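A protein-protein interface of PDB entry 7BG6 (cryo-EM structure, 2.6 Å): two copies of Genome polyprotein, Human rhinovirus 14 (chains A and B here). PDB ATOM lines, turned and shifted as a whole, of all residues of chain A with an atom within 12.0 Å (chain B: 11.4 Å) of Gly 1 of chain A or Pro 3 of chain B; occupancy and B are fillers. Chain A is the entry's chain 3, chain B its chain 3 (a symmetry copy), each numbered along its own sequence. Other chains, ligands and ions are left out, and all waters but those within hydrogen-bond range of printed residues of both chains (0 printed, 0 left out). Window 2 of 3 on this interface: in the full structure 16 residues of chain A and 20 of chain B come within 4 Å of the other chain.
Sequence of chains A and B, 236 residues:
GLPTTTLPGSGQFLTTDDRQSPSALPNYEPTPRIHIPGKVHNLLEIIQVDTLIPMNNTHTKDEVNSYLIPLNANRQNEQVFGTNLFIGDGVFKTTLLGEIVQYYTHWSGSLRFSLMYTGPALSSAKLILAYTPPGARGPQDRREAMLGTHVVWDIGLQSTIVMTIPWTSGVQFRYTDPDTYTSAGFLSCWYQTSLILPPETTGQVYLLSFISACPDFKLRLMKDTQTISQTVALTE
The backbone NH (N) of Leu 2 of chain A lies within hydrogen-bond range of the backbone carbonyl oxygen (O) of Pro 3 of chain B (3.1 Å). O of Leu 2 of chain A lies within hydrogen-bond range of N of Thr 5 of chain B (2.9 Å). The backbone NH of Thr 4 of chain A lies within hydrogen-bond range of the backbone carbonyl oxygen of Thr 5 of chain B (2.7 Å). The backbone carbonyl oxygen (O) of Thr 4 of chain A is in hydrogen-bond range of the backbone NH (N) of Leu 7 of chain B (2.6 Å).
Gly 1 of chain A touches Pro 3 of chain B (CA to O, 3.5 Å). Leu 2 of chain B touches Leu 2 of chain A (CD2 to CD2, 3.9 Å). Thr 4 of chain B touches Leu 2 of chain A (CA to O, 3.2 Å). Pro 3 of chain A touches Thr 5 of chain B. CD2 of Leu 7 of chain B touches CB of Pro 3 of chain A, at 3.8 Å. CG2 of Thr 4 of chain B touches CG2 of Thr 4 of chain A, 3.8 Å away. CA of Thr 6 of chain B touches O of Thr 4 of chain A, at 3.2 Å. Thr 5 of chain A touches Leu 7 of chain B (OG1 to CB, 3.3 Å).
Leu 2 of chain A touches four residues of chain B. Of the printed residues of chain B, Thr 4 of chain A touches Thr 4, Thr 5, Thr 6 and Leu 7. Printed residues of chain B within 4 Å of Thr 5 of chain A: Leu 7. No residue of chain A comes within 4 Å of Gly 1 of chain B. Pro 3 of chain B touches two residues of chain A. Thr 4 of chain B touches just these residues of chain A: Leu 2 (3.2 Å) and Thr 4 (3.8 Å). Thr 5 of chain B touches three residues of chain A. Of the printed residues of chain A, Leu 7 of chain B touches Pro 3 (3.8 Å), Thr 4 (2.6 Å) and Thr 5 (3.3 Å). The nearest residue of chain A that does not touch Pro 3 of chain B is Pro 3 of chain A (6.0 Å). The nearest printed residue of chain B that does not touch Thr 5 of chain A is Thr 6 of chain B (5.1 Å).
Hydrophobic or aromatic side chains of chain B that line the printed part of chain A: Leu 2 and Leu 7. Hydrophobic or aromatic side chains of chain A that line the printed part of chain B: Leu 2 and Pro 3. Along chain A the printed residues that touch a printed residue of chain B span positions 1 to 5.
Gly 1 of chain A touches Pro 3 of chain B, but with the chains exchanged Pro 3 of chain A does not touch Gly 1 of chain B (12.1 Å). Leu 2 of chain A touches Thr 4 of chain B, but with the chains exchanged Thr 4 of chain A does not touch Leu 2 of chain B (6.5 Å). Leu 2 of chain A touches Thr 5 of chain B, but with the chains exchanged Thr 5 of chain A does not touch Leu 2 of chain B (10.8 Å). Thr 4 of chain A touches Thr 5 of chain B, but with the chains exchanged Thr 5 of chain A does not touch Thr 4 of chain B (7.6 Å). Positions printed for both chains: 1, 2, 3, 4, 5 and 6.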
ATOM      1  N   GLY A   1     -23.893   9.618 -20.412  1.00  0.00           N
ATOM      2  CA  GLY A   1     -24.167   8.547 -21.414  1.00  0.00           C
ATOM      3  C   GLY A   1     -24.327   7.181 -20.753  1.00  0.00           C
ATOM      4  O   GLY A   1     -23.701   6.906 -19.730  1.00  0.00           O
ATOM      5  N   LEU A   2     -25.170   6.339 -21.362  1.00  0.00           N
ATOM      6  CA  LEU A   2     -25.535   5.042 -20.817  1.00  0.00           C
ATOM      7  C   LEU A   2     -24.305   4.137 -20.766  1.00  0.00           C
ATOM      8  O   LEU A   2     -23.668   3.898 -21.790  1.00  0.00           O
ATOM      9  CB  LEU A   2     -26.645   4.433 -21.683  1.00  0.00           C
ATOM     10  CG  LEU A   2     -27.134   3.042 -21.275  1.00  0.00           C
ATOM     11  CD1 LEU A   2     -27.876   3.085 -19.946  1.00  0.00           C
ATOM     12  CD2 LEU A   2     -28.022   2.444 -22.355  1.00  0.00           C
ATOM     13  N   PRO A   3     -23.927   3.626 -19.570  1.00  0.00           N
ATOM     14  CA  PRO A   3     -22.838   2.655 -19.447  1.00  0.00           C
ATOM     15  C   PRO A   3     -23.204   1.335 -20.121  1.00  0.00           C
ATOM     16  O   PRO A   3     -24.272   0.780 -19.871  1.00  0.00           O
ATOM     17  CB  PRO A   3     -22.693   2.451 -17.929  1.00  0.00           C
ATOM     18  CG  PRO A   3     -23.373   3.654 -17.315  1.00  0.00           C
ATOM     19  CD  PRO A   3     -24.506   3.981 -18.265  1.00  0.00           C
ATOM     20  N   THR A   4     -22.302   0.856 -20.984  1.00  0.00           N
ATOM     21  CA  THR A   4     -22.511  -0.363 -21.749  1.00  0.00           C
ATOM     22  C   THR A   4     -21.310  -1.289 -21.579  1.00  0.00           C
ATOM     23  O   THR A   4     -20.227  -0.844 -21.208  1.00  0.00           O
ATOM     24  CB  THR A   4     -22.742  -0.055 -23.235  1.00  0.00           C
ATOM     25  OG1 THR A   4     -21.615   0.670 -23.729  1.00  0.00           O
ATOM     26  CG2 THR A   4     -24.010   0.726 -23.495  1.00  0.00           C
ATOM     27  N   THR A   5     -21.524  -2.581 -21.850  1.00  0.00           N
ATOM     28  CA  THR A   5     -20.443  -3.550 -21.931  1.00  0.00           C
ATOM     29  C   THR A   5     -20.624  -4.384 -23.196  1.00  0.00           C
ATOM     30  O   THR A   5     -21.657  -5.026 -23.376  1.00  0.00           O
ATOM     31  CB  THR A   5     -20.340  -4.394 -20.653  1.00  0.00           C
ATOM     32  OG1 THR A   5     -20.120  -3.511 -19.552  1.00  0.00           O
ATOM     33  CG2 THR A   5     -19.228  -5.419 -20.705  1.00  0.00           C
ATOM     34  N   THR A   6     -19.608  -4.358 -24.067  1.00  0.00           N
ATOM     35  CA  THR A   6     -19.670  -5.061 -25.338  1.00  0.00           C
ATOM     36  C   THR A   6     -19.381  -6.543 -25.118  1.00  0.00           C
ATOM     37  O   THR A   6     -18.342  -6.905 -24.569  1.00  0.00           O
ATOM     38  CB  THR A   6     -18.747  -4.424 -26.388  1.00  0.00           C
ATOM     39  OG1 THR A   6     -17.393  -4.563 -25.958  1.00  0.00           O
ATOM     40  CG2 THR A   6     -19.059  -2.967 -26.654  1.00  0.00           C
ATOM     41  N   GLY B   1     -27.912   9.338 -32.476  1.00  0.00           N
ATOM     42  CA  GLY B   1     -27.664   8.015 -31.831  1.00  0.00           C
ATOM     43  C   GLY B   1     -27.408   8.154 -30.334  1.00  0.00           C
ATOM     44  O   GLY B   1     -26.853   9.158 -29.887  1.00  0.00           O
ATOM     45  N   LEU B   2     -27.817   7.127 -29.580  1.00  0.00           N
ATOM     46  CA  LEU B   2     -27.759   7.132 -28.127  1.00  0.00           C
ATOM     47  C   LEU B   2     -26.304   7.191 -27.665  1.00  0.00           C
ATOM     48  O   LEU B   2     -25.505   6.327 -28.024  1.00  0.00           O
ATOM     49  CB  LEU B   2     -28.468   5.879 -27.597  1.00  0.00           C
ATOM     50  CG  LEU B   2     -28.476   5.700 -26.078  1.00  0.00           C
ATOM     51  CD1 LEU B   2     -29.339   6.755 -25.401  1.00  0.00           C
ATOM     52  CD2 LEU B   2     -28.957   4.306 -25.701  1.00  0.00           C
ATOM     53  N   PRO B   3     -25.917   8.219 -26.874  1.00  0.00           N
ATOM     54  CA  PRO B   3     -24.577   8.288 -26.287  1.00  0.00           C
ATOM     55  C   PRO B   3     -24.367   7.166 -25.273  1.00  0.00           C
ATOM     56  O   PRO B   3     -25.189   6.964 -24.382  1.00  0.00           O
ATOM     57  CB  PRO B   3     -24.554   9.652 -25.576  1.00  0.00           C
ATOM     58  CG  PRO B   3     -25.686  10.431 -26.208  1.00  0.00           C
ATOM     59  CD  PRO B   3     -26.736   9.390 -26.528  1.00  0.00           C
ATOM     60  N   THR B   4     -23.256   6.439 -25.437  1.00  0.00           N
ATOM     61  CA  THR B   4     -22.925   5.304 -24.591  1.00  0.00           C
ATOM     62  C   THR B   4     -21.501   5.457 -24.058  1.00  0.00           C
ATOM     63  O   THR B   4     -20.701   6.197 -24.623  1.00  0.00           O
ATOM     64  CB  THR B   4     -23.068   3.980 -25.355  1.00  0.00           C
ATOM     65  OG1 THR B   4     -22.220   4.025 -26.504  1.00  0.00           O
ATOM     66  CG2 THR B   4     -24.490   3.682 -25.775  1.00  0.00           C
ATOM     67  N   THR B   5     -21.208   4.750 -22.961  1.00  0.00           N
ATOM     68  CA  THR B   5     -19.853   4.632 -22.450  1.00  0.00           C
ATOM     69  C   THR B   5     -19.572   3.164 -22.141  1.00  0.00           C
ATOM     70  O   THR B   5     -20.279   2.548 -21.345  1.00  0.00           O
ATOM     71  CB  THR B   5     -19.612   5.564 -21.255  1.00  0.00           C
ATOM     72  OG1 THR B   5     -19.854   6.906 -21.681  1.00  0.00           O
ATOM     73  CG2 THR B   5     -18.211   5.460 -20.694  1.00  0.00           C
ATOM     74  N   THR B   6     -18.534   2.616 -22.784  1.00  0.00           N
ATOM     75  CA  THR B   6     -18.188   1.213 -22.627  1.00  0.00           C
ATOM     76  C   THR B   6     -17.421   1.018 -21.322  1.00  0.00           C
ATOM     77  O   THR B   6     -16.395   1.658 -21.096  1.00  0.00           O
ATOM     78  CB  THR B   6     -17.432   0.669 -23.849  1.00  0.00           C
ATOM     79  OG1 THR B   6     -16.179   1.347 -23.955  1.00  0.00           O
ATOM     80  CG2 THR B   6     -18.207   0.809 -25.141  1.00  0.00           C
ATOM     81  N   LEU B   7     -17.944   0.127 -20.472  1.00  0.00           N
ATOM     82  CA  LEU B   7     -17.334  -0.198 -19.193  1.00  0.00           C
ATOM     83  C   LEU B   7     -16.082  -1.039 -19.432  1.00  0.00           C
ATOM     84  O   LEU B   7     -15.921  -1.616 -20.506  1.00  0.00           O
ATOM     85  CB  LEU B   7     -18.345  -0.971 -18.338  1.00  0.00           C
ATOM     86  CG  LEU B   7     -19.606  -0.210 -17.929  1.00  0.00           C
ATOM     87  CD1 LEU B   7     -20.478  -1.076 -17.036  1.00  0.00           C
ATOM     88  CD2 LEU B   7     -19.261   1.094 -17.224  1.00  0.00           C
